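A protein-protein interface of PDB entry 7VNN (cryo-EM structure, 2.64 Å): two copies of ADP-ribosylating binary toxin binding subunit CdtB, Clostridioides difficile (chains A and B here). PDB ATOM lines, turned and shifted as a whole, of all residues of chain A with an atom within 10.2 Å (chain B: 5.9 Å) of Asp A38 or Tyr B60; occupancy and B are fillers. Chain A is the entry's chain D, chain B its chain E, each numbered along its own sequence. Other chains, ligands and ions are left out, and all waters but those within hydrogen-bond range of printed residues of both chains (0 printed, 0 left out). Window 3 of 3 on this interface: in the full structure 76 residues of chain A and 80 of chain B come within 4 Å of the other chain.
The side-chain carboxylate of Glu B338 lies within hydrogen-bond range of the backbone NH of Asp A38 (2.8 Å). The side-chain carboxylate (OE2) of Glu B338 lies within hydrogen-bond range of the side-chain hydroxyl (OH) of Tyr A53 (3.1 Å). OD1 of Asp A38 is in hydrogen-bond range of OH of Tyr B60 (3.2 Å).
The side-chain amide oxygen (OD1) of Asn B59 is in hydrogen-bond range of the backbone NH (N) of Leu B61 (2.9 Å). O of Leu A39 is in hydrogen-bond range of OH of Tyr A73, at 2.6 Å.
CG of Glu B338 touches O of Ile A36, at 3.6 Å. CA of Lys A37 touches OE1 of Glu B338, 3.4 Å away. Asp A38 touches Leu B61 (OD1 to CD1, 3.5 Å). Leu A39 touches Leu B61.
Of chain B, only Tyr B60 (3.2 Å), Leu B61 (3.5 Å) and Glu B338 (2.8 Å) come within 4 Å of Asp A38. Of chain A, only Asp A38 (3.2 Å) comes within 4 Å of Tyr B60. Asp B27 touches none of the printed residues of chain A. No residue of chain A comes within 4 Å of Glu B30. Leu B61 touches two residues of chain A. Of the printed residues of chain B, Leu A39 touches Leu B61 (3.96 Å). Printed residues of chain B within 4 Å of Tyr A53: Glu B338 (3.1 Å). Tyr A73 touches none of the printed residues of chain B. The nearest residue of chain A that does not touch Tyr B60 is Leu A39 (6.7 Å).
Printed residues of chain A that touch a printed residue of chain B: Ile A36, Lys A37, Asp A38, Leu A39 and Tyr A53. Of the 16 printed residues of chain B, 3 touch a printed residue of chain A. Along chain B the printed residues that touch a printed residue of chain A span positions 60 to 338. Among the printed residues, 7 pairs touch across the chains. Among the printed residues, no Asp or Glu carboxylate lies within 4 Å of a Lys or Arg side-chain nitrogen of the other chain.
No position is printed for both chains. Of the 7 pairs that touch across the chains among the printed residues, none has its exchanged pair printed and touching as well.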
ATOM      1  N   THR A  35      12.191 -33.459  20.998  1.00  0.00           N
ATOM      2  CA  THR A  35      12.674 -32.138  20.626  1.00  0.00           C
ATOM      3  C   THR A  35      11.720 -31.104  21.203  1.00  0.00           C
ATOM      4  O   THR A  35      10.618 -31.432  21.649  1.00  0.00           O
ATOM      5  CB  THR A  35      12.797 -31.977  19.106  1.00  0.00           C
ATOM      6  OG1 THR A  35      13.481 -30.755  18.811  1.00  0.00           O
ATOM      7  CG2 THR A  35      11.426 -31.949  18.462  1.00  0.00           C
ATOM      8  N   ILE A  36      12.156 -29.849  21.196  1.00  0.00           N
ATOM      9  CA  ILE A  36      11.409 -28.755  21.805  1.00  0.00           C
ATOM     10  C   ILE A  36      10.885 -27.849  20.701  1.00  0.00           C
ATOM     11  O   ILE A  36      11.661 -27.352  19.874  1.00  0.00           O
ATOM     12  CB  ILE A  36      12.274 -27.962  22.796  1.00  0.00           C
ATOM     13  CG1 ILE A  36      12.854 -28.887  23.868  1.00  0.00           C
ATOM     14  CG2 ILE A  36      11.458 -26.848  23.431  1.00  0.00           C
ATOM     15  CD1 ILE A  36      11.839 -29.387  24.865  1.00  0.00           C
ATOM     16  N   LYS A  37       9.571 -27.638  20.683  1.00  0.00           N
ATOM     17  CA  LYS A  37       8.958 -26.617  19.843  1.00  0.00           C
ATOM     18  C   LYS A  37       7.862 -25.930  20.639  1.00  0.00           C
ATOM     19  O   LYS A  37       7.034 -26.600  21.262  1.00  0.00           O
ATOM     20  CB  LYS A  37       8.392 -27.206  18.547  1.00  0.00           C
ATOM     21  CG  LYS A  37       7.709 -28.546  18.700  1.00  0.00           C
ATOM     22  CD  LYS A  37       7.126 -29.007  17.372  1.00  0.00           C
ATOM     23  CE  LYS A  37       8.190 -29.060  16.289  1.00  0.00           C
ATOM     24  NZ  LYS A  37       7.631 -29.496  14.983  1.00  0.00           N
ATOM     25  N   ASP A  38       7.864 -24.595  20.612  1.00  0.00           N
ATOM     26  CA  ASP A  38       6.951 -23.779  21.415  1.00  0.00           C
ATOM     27  C   ASP A  38       7.059 -24.121  22.900  1.00  0.00           C
ATOM     28  O   ASP A  38       6.067 -24.119  23.630  1.00  0.00           O
ATOM     29  CB  ASP A  38       5.508 -23.911  20.928  1.00  0.00           C
ATOM     30  CG  ASP A  38       5.200 -22.986  19.769  1.00  0.00           C
ATOM     31  OD1 ASP A  38       6.002 -22.064  19.517  1.00  0.00           O
ATOM     32  OD2 ASP A  38       4.157 -23.176  19.111  1.00  0.00           O
ATOM     33  N   LEU A  39       8.282 -24.419  23.344  1.00  0.00           N
ATOM     34  CA  LEU A  39       8.585 -24.693  24.751  1.00  0.00           C
ATOM     35  C   LEU A  39       7.774 -25.870  25.294  1.00  0.00           C
ATOM     36  O   LEU A  39       7.370 -25.882  26.457  1.00  0.00           O
ATOM     37  CB  LEU A  39       8.374 -23.446  25.611  1.00  0.00           C
ATOM     38  CG  LEU A  39       9.064 -22.174  25.117  1.00  0.00           C
ATOM     39  CD1 LEU A  39       8.751 -21.003  26.029  1.00  0.00           C
ATOM     40  CD2 LEU A  39      10.560 -22.392  25.014  1.00  0.00           C
ATOM     41  N   ILE A  40       7.535 -26.869  24.449  1.00  0.00           N
ATOM     42  CA  ILE A  40       6.854 -28.096  24.852  1.00  0.00           C
ATOM     43  C   ILE A  40       7.578 -29.275  24.220  1.00  0.00           C
ATOM     44  O   ILE A  40       7.874 -29.257  23.021  1.00  0.00           O
ATOM     45  CB  ILE A  40       5.366 -28.097  24.450  1.00  0.00           C
ATOM     46  CG1 ILE A  40       4.607 -26.990  25.182  1.00  0.00           C
ATOM     47  CG2 ILE A  40       4.733 -29.444  24.740  1.00  0.00           C
ATOM     48  CD1 ILE A  40       3.205 -26.764  24.661  1.00  0.00           C
ATOM     49  N   ALA A  41       7.863 -30.297  25.023  1.00  0.00           N
ATOM     50  CA  ALA A  41       8.520 -31.490  24.508  1.00  0.00           C
ATOM     51  C   ALA A  41       7.546 -32.308  23.673  1.00  0.00           C
ATOM     52  O   ALA A  41       6.413 -32.562  24.090  1.00  0.00           O
ATOM     53  CB  ALA A  41       9.070 -32.332  25.658  1.00  0.00           C
ATOM     54  N   VAL A  42       7.993 -32.723  22.487  1.00  0.00           N
ATOM     55  CA  VAL A  42       7.181 -33.505  21.567  1.00  0.00           C
ATOM     56  C   VAL A  42       7.994 -34.705  21.103  1.00  0.00           C
ATOM     57  O   VAL A  42       9.220 -34.735  21.219  1.00  0.00           O
ATOM     58  CB  VAL A  42       6.707 -32.675  20.354  1.00  0.00           C
ATOM     59  CG1 VAL A  42       5.838 -31.513  20.809  1.00  0.00           C
ATOM     60  CG2 VAL A  42       7.898 -32.174  19.557  1.00  0.00           C
ATOM     61  N   TYR A  53      15.750 -29.183  13.323  1.00  0.00           N
ATOM     62  CA  TYR A  53      15.593 -29.598  14.709  1.00  0.00           C
ATOM     63  C   TYR A  53      16.596 -30.690  15.064  1.00  0.00           C
ATOM     64  O   TYR A  53      16.933 -31.548  14.245  1.00  0.00           O
ATOM     65  CB  TYR A  53      14.172 -30.095  14.957  1.00  0.00           C
ATOM     66  CG  TYR A  53      13.125 -29.008  14.928  1.00  0.00           C
ATOM     67  CD1 TYR A  53      12.872 -28.231  16.048  1.00  0.00           C
ATOM     68  CD2 TYR A  53      12.389 -28.761  13.780  1.00  0.00           C
ATOM     69  CE1 TYR A  53      11.913 -27.239  16.026  1.00  0.00           C
ATOM     70  CE2 TYR A  53      11.429 -27.771  13.748  1.00  0.00           C
ATOM     71  CZ  TYR A  53      11.195 -27.014  14.874  1.00  0.00           C
ATOM     72  OH  TYR A  53      10.239 -26.026  14.846  1.00  0.00           O
ATOM     73  N   TYR A  73      15.416 -30.161  30.591  1.00  0.00           N
ATOM     74  CA  TYR A  73      14.475 -29.306  29.873  1.00  0.00           C
ATOM     75  C   TYR A  73      15.046 -27.912  29.654  1.00  0.00           C
ATOM     76  O   TYR A  73      14.894 -27.341  28.567  1.00  0.00           O
ATOM     77  CB  TYR A  73      13.147 -29.223  30.621  1.00  0.00           C
ATOM     78  CG  TYR A  73      12.156 -28.304  29.945  1.00  0.00           C
ATOM     79  CD1 TYR A  73      11.411 -28.737  28.858  1.00  0.00           C
ATOM     80  CD2 TYR A  73      11.980 -27.000  30.384  1.00  0.00           C
ATOM     81  CE1 TYR A  73      10.514 -27.900  28.230  1.00  0.00           C
ATOM     82  CE2 TYR A  73      11.087 -26.156  29.762  1.00  0.00           C
ATOM     83  CZ  TYR A  73      10.357 -26.609  28.687  1.00  0.00           C
ATOM     84  OH  TYR A  73       9.463 -25.767  28.069  1.00  0.00           O
ATOM     85  N   ALA A  76      17.654 -28.263  26.841  1.00  0.00           N
ATOM     86  CA  ALA A  76      17.094 -28.591  25.534  1.00  0.00           C
ATOM     87  C   ALA A  76      16.299 -27.428  24.956  1.00  0.00           C
ATOM     88  O   ALA A  76      16.439 -27.099  23.774  1.00  0.00           O
ATOM     89  CB  ALA A  76      16.219 -29.839  25.638  1.00  0.00           C
ATOM     90  N   SER A  77      15.464 -26.788  25.776  1.00  0.00           N
ATOM     91  CA  SER A  77      14.603 -25.720  25.289  1.00  0.00           C
ATOM     92  C   SER A  77      15.331 -24.394  25.134  1.00  0.00           C
ATOM     93  O   SER A  77      14.779 -23.469  24.531  1.00  0.00           O
ATOM     94  CB  SER A  77      13.408 -25.544  26.229  1.00  0.00           C
ATOM     95  OG  SER A  77      13.826 -25.101  27.507  1.00  0.00           O
ATOM     96  N   GLY A  78      16.552 -24.281  25.648  1.00  0.00           N
ATOM     97  CA  GLY A  78      17.248 -23.012  25.613  1.00  0.00           C
ATOM     98  C   GLY A  78      16.644 -21.943  26.490  1.00  0.00           C
ATOM     99  O   GLY A  78      16.686 -20.764  26.131  1.00  0.00           O
ATOM    100  N   SER A  79      16.126 -22.352  27.651  1.00  0.00           N
ATOM    101  CA  SER A  79      15.560 -21.382  28.622  1.00  0.00           C
ATOM    102  C   SER A  79      16.630 -21.038  29.661  1.00  0.00           C
ATOM    103  O   SER A  79      16.307 -21.061  30.864  1.00  0.00           O
ATOM    104  CB  SER A  79      14.325 -21.941  29.273  1.00  0.00           C
ATOM    105  OG  SER A  79      13.368 -22.319  28.294  1.00  0.00           O
ATOM    106  N   ARG A  89      23.461 -27.223  24.556  1.00  0.00           N
ATOM    107  CA  ARG A  89      22.012 -27.302  24.670  1.00  0.00           C
ATOM    108  C   ARG A  89      21.488 -28.729  24.586  1.00  0.00           C
ATOM    109  O   ARG A  89      20.305 -28.950  24.865  1.00  0.00           O
ATOM    110  CB  ARG A  89      21.350 -26.435  23.600  1.00  0.00           C
ATOM    111  CG  ARG A  89      21.561 -24.952  23.826  1.00  0.00           C
ATOM    112  CD  ARG A  89      20.923 -24.120  22.739  1.00  0.00           C
ATOM    113  NE  ARG A  89      19.474 -24.248  22.744  1.00  0.00           N
ATOM    114  CZ  ARG A  89      18.675 -23.728  21.825  1.00  0.00           C
ATOM    115  NH1 ARG A  89      19.153 -23.016  20.818  1.00  0.00           N
ATOM    116  NH2 ARG A  89      17.363 -23.924  21.918  1.00  0.00           N
ATOM    117  N   THR B  20       2.110 -17.069  25.672  1.00  0.00           N
ATOM    118  CA  THR B  20       3.003 -18.182  25.979  1.00  0.00           C
ATOM    119  C   THR B  20       4.108 -17.784  26.950  1.00  0.00           C
ATOM    120  O   THR B  20       4.369 -18.509  27.915  1.00  0.00           O
ATOM    121  CB  THR B  20       3.608 -18.740  24.692  1.00  0.00           C
ATOM    122  OG1 THR B  20       2.560 -19.043  23.764  1.00  0.00           O
ATOM    123  CG2 THR B  20       4.399 -20.002  24.981  1.00  0.00           C
ATOM    124  N   ASP B  21       4.760 -16.645  26.724  1.00  0.00           N
ATOM    125  CA  ASP B  21       5.873 -16.217  27.559  1.00  0.00           C
ATOM    126  C   ASP B  21       5.429 -15.458  28.800  1.00  0.00           C
ATOM    127  O   ASP B  21       6.277 -15.103  29.626  1.00  0.00           O
ATOM    128  CB  ASP B  21       6.846 -15.355  26.745  1.00  0.00           C
ATOM    129  CG  ASP B  21       6.148 -14.244  25.994  1.00  0.00           C
ATOM    130  OD1 ASP B  21       4.921 -14.101  26.149  1.00  0.00           O
ATOM    131  OD2 ASP B  21       6.826 -13.514  25.245  1.00  0.00           O
ATOM    132  N   PRO B  26      -0.359 -10.709  23.998  1.00  0.00           N
ATOM    133  CA  PRO B  26      -0.711 -11.939  23.281  1.00  0.00           C
ATOM    134  C   PRO B  26       0.228 -12.219  22.116  1.00  0.00           C
ATOM    135  O   PRO B  26       0.855 -11.324  21.547  1.00  0.00           O
ATOM    136  CB  PRO B  26      -2.138 -11.669  22.794  1.00  0.00           C
ATOM    137  CG  PRO B  26      -2.653 -10.613  23.712  1.00  0.00           C
ATOM    138  CD  PRO B  26      -1.476  -9.756  24.039  1.00  0.00           C
ATOM    139  N   ASP B  27       0.311 -13.507  21.767  1.00  0.00           N
ATOM    140  CA  ASP B  27       1.273 -13.963  20.767  1.00  0.00           C
ATOM    141  C   ASP B  27       1.006 -13.341  19.401  1.00  0.00           C
ATOM    142  O   ASP B  27       1.943 -12.936  18.701  1.00  0.00           O
ATOM    143  CB  ASP B  27       1.234 -15.486  20.671  1.00  0.00           C
ATOM    144  CG  ASP B  27       1.753 -16.165  21.923  1.00  0.00           C
ATOM    145  OD1 ASP B  27       2.614 -15.577  22.608  1.00  0.00           O
ATOM    146  OD2 ASP B  27       1.295 -17.287  22.224  1.00  0.00           O
ATOM    147  N   SER B  28      -0.264 -13.270  19.001  1.00  0.00           N
ATOM    148  CA  SER B  28      -0.598 -12.712  17.695  1.00  0.00           C
ATOM    149  C   SER B  28      -0.223 -11.239  17.610  1.00  0.00           C
ATOM    150  O   SER B  28       0.231 -10.766  16.559  1.00  0.00           O
ATOM    151  CB  SER B  28      -2.084 -12.914  17.402  1.00  0.00           C
ATOM    152  OG  SER B  28      -2.886 -12.519  18.500  1.00  0.00           O
ATOM    153  N   GLU B  30       2.274  -9.791  19.209  1.00  0.00           N
ATOM    154  CA  GLU B  30       3.727  -9.737  19.090  1.00  0.00           C
ATOM    155  C   GLU B  30       4.177 -10.087  17.679  1.00  0.00           C
ATOM    156  O   GLU B  30       5.099  -9.463  17.142  1.00  0.00           O
ATOM    157  CB  GLU B  30       4.371 -10.680  20.105  1.00  0.00           C
ATOM    158  CG  GLU B  30       4.206 -10.247  21.547  1.00  0.00           C
ATOM    159  CD  GLU B  30       5.312 -10.763  22.444  1.00  0.00           C
ATOM    160  OE1 GLU B  30       6.474 -10.362  22.246  1.00  0.00           O
ATOM    161  OE2 GLU B  30       5.022 -11.572  23.346  1.00  0.00           O
ATOM    162  N   ARG B  31       3.544 -11.089  17.067  1.00  0.00           N
ATOM    163  CA  ARG B  31       3.918 -11.469  15.709  1.00  0.00           C
ATOM    164  C   ARG B  31       3.583 -10.367  14.712  1.00  0.00           C
ATOM    165  O   ARG B  31       4.434  -9.963  13.911  1.00  0.00           O
ATOM    166  CB  ARG B  31       3.225 -12.775  15.316  1.00  0.00           C
ATOM    167  CG  ARG B  31       3.866 -14.025  15.889  1.00  0.00           C
ATOM    168  CD  ARG B  31       3.364 -15.268  15.174  1.00  0.00           C
ATOM    169  NE  ARG B  31       1.927 -15.451  15.335  1.00  0.00           N
ATOM    170  CZ  ARG B  31       1.367 -16.188  16.283  1.00  0.00           C
ATOM    171  NH1 ARG B  31       2.097 -16.836  17.177  1.00  0.00           N
ATOM    172  NH2 ARG B  31       0.041 -16.276  16.339  1.00  0.00           N
ATOM    173  N   SER B  58       8.161  -8.148  18.590  1.00  0.00           N
ATOM    174  CA  SER B  58       9.059  -8.773  19.552  1.00  0.00           C
ATOM    175  C   SER B  58       8.897 -10.286  19.473  1.00  0.00           C
ATOM    176  O   SER B  58       8.055 -10.806  18.737  1.00  0.00           O
ATOM    177  CB  SER B  58       8.792  -8.255  20.966  1.00  0.00           C
ATOM    178  OG  SER B  58       7.485  -8.585  21.395  1.00  0.00           O
ATOM    179  N   ASN B  59       9.722 -10.988  20.245  1.00  0.00           N
ATOM    180  CA  ASN B  59       9.693 -12.443  20.295  1.00  0.00           C
ATOM    181  C   ASN B  59       8.518 -12.894  21.152  1.00  0.00           C
ATOM    182  O   ASN B  59       8.434 -12.544  22.333  1.00  0.00           O
ATOM    183  CB  ASN B  59      11.012 -12.969  20.861  1.00  0.00           C
ATOM    184  CG  ASN B  59      11.197 -14.458  20.643  1.00  0.00           C
ATOM    185  OD1 ASN B  59      10.234 -15.195  20.439  1.00  0.00           O
ATOM    186  ND2 ASN B  59      12.445 -14.907  20.688  1.00  0.00           N
ATOM    187  N   TYR B  60       7.614 -13.675  20.564  1.00  0.00           N
ATOM    188  CA  TYR B  60       6.445 -14.146  21.296  1.00  0.00           C
ATOM    189  C   TYR B  60       6.731 -15.378  22.145  1.00  0.00           C
ATOM    190  O   TYR B  60       5.843 -15.821  22.881  1.00  0.00           O
ATOM    191  CB  TYR B  60       5.289 -14.420  20.327  1.00  0.00           C
ATOM    192  CG  TYR B  60       5.313 -15.769  19.642  1.00  0.00           C
ATOM    193  CD1 TYR B  60       5.983 -15.945  18.440  1.00  0.00           C
ATOM    194  CD2 TYR B  60       4.642 -16.859  20.180  1.00  0.00           C
ATOM    195  CE1 TYR B  60       5.998 -17.168  17.805  1.00  0.00           C
ATOM    196  CE2 TYR B  60       4.656 -18.086  19.553  1.00  0.00           C
ATOM    197  CZ  TYR B  60       5.334 -18.234  18.366  1.00  0.00           C
ATOM    198  OH  TYR B  60       5.348 -19.456  17.736  1.00  0.00           O
ATOM    199  N   LEU B  61       7.935 -15.942  22.063  1.00  0.00           N
ATOM    200  CA  LEU B  61       8.350 -17.039  22.927  1.00  0.00           C
ATOM    201  C   LEU B  61       9.359 -16.598  23.978  1.00  0.00           C
ATOM    202  O   LEU B  61       9.883 -17.440  24.712  1.00  0.00           O
ATOM    203  CB  LEU B  61       8.933 -18.183  22.097  1.00  0.00           C
ATOM    204  CG  LEU B  61       7.952 -19.005  21.265  1.00  0.00           C
ATOM    205  CD1 LEU B  61       8.673 -20.163  20.601  1.00  0.00           C
ATOM    206  CD2 LEU B  61       6.805 -19.503  22.127  1.00  0.00           C
ATOM    207  N   GLU B  62       9.642 -15.301  24.067  1.00  0.00           N
ATOM    208  CA  GLU B  62      10.639 -14.778  24.989  1.00  0.00           C
ATOM    209  C   GLU B  62      10.076 -13.556  25.693  1.00  0.00           C
ATOM    210  O   GLU B  62       9.528 -12.661  25.043  1.00  0.00           O
ATOM    211  CB  GLU B  62      11.931 -14.417  24.253  1.00  0.00           C
ATOM    212  CG  GLU B  62      13.043 -13.929  25.155  1.00  0.00           C
ATOM    213  CD  GLU B  62      13.514 -14.995  26.119  1.00  0.00           C
ATOM    214  OE1 GLU B  62      13.949 -16.068  25.652  1.00  0.00           O
ATOM    215  OE2 GLU B  62      13.448 -14.760  27.343  1.00  0.00           O
ATOM    216  N   THR B  65      13.061  -9.929  24.952  1.00  0.00           N
ATOM    217  CA  THR B  65      13.567 -10.133  23.597  1.00  0.00           C
ATOM    218  C   THR B  65      15.002  -9.643  23.453  1.00  0.00           C
ATOM    219  O   THR B  65      15.838 -10.320  22.843  1.00  0.00           O
ATOM    220  CB  THR B  65      12.659  -9.425  22.593  1.00  0.00           C
ATOM    221  OG1 THR B  65      11.335  -9.964  22.686  1.00  0.00           O
ATOM    222  CG2 THR B  65      13.173  -9.610  21.179  1.00  0.00           C
ATOM    223  N   ASP B  72       9.356  -7.128  27.590  1.00  0.00           N
ATOM    224  CA  ASP B  72       8.794  -6.502  26.397  1.00  0.00           C
ATOM    225  C   ASP B  72       7.701  -5.505  26.753  1.00  0.00           C
ATOM    226  O   ASP B  72       7.665  -4.393  26.213  1.00  0.00           O
ATOM    227  CB  ASP B  72       8.248  -7.574  25.456  1.00  0.00           C
ATOM    228  CG  ASP B  72       9.337  -8.424  24.848  1.00  0.00           C
ATOM    229  OD1 ASP B  72      10.498  -7.967  24.807  1.00  0.00           O
ATOM    230  OD2 ASP B  72       9.034  -9.553  24.412  1.00  0.00           O
ATOM    231  N   GLU B 338      13.570 -22.280  16.421  1.00  0.00           N
ATOM    232  CA  GLU B 338      12.791 -21.792  17.549  1.00  0.00           C
ATOM    233  C   GLU B 338      13.152 -20.370  17.950  1.00  0.00           C
ATOM    234  O   GLU B 338      12.625 -19.869  18.947  1.00  0.00           O
ATOM    235  CB  GLU B 338      12.958 -22.726  18.751  1.00  0.00           C
ATOM    236  CG  GLU B 338      12.261 -24.061  18.589  1.00  0.00           C
ATOM    237  CD  GLU B 338      10.761 -23.918  18.448  1.00  0.00           C
ATOM    238  OE1 GLU B 338      10.119 -23.423  19.395  1.00  0.00           O
ATOM    239  OE2 GLU B 338      10.221 -24.303  17.389  1.00  0.00           O
ATOM    240  N   LYS B 340      12.374 -16.897  17.403  1.00  0.00           N
ATOM    241  CA  LYS B 340      11.236 -16.216  16.804  1.00  0.00           C
ATOM    242  C   LYS B 340      11.377 -14.702  16.808  1.00  0.00           C
ATOM    243  O   LYS B 340      10.399 -14.001  16.529  1.00  0.00           O
ATOM    244  CB  LYS B 340       9.946 -16.622  17.518  1.00  0.00           C
ATOM    245  CG  LYS B 340       9.770 -18.122  17.667  1.00  0.00           C
ATOM    246  CD  LYS B 340       9.596 -18.793  16.315  1.00  0.00           C
ATOM    247  CE  LYS B 340       9.282 -20.268  16.472  1.00  0.00           C
ATOM    248  NZ  LYS B 340       9.122 -20.945  15.156  1.00  0.00           N
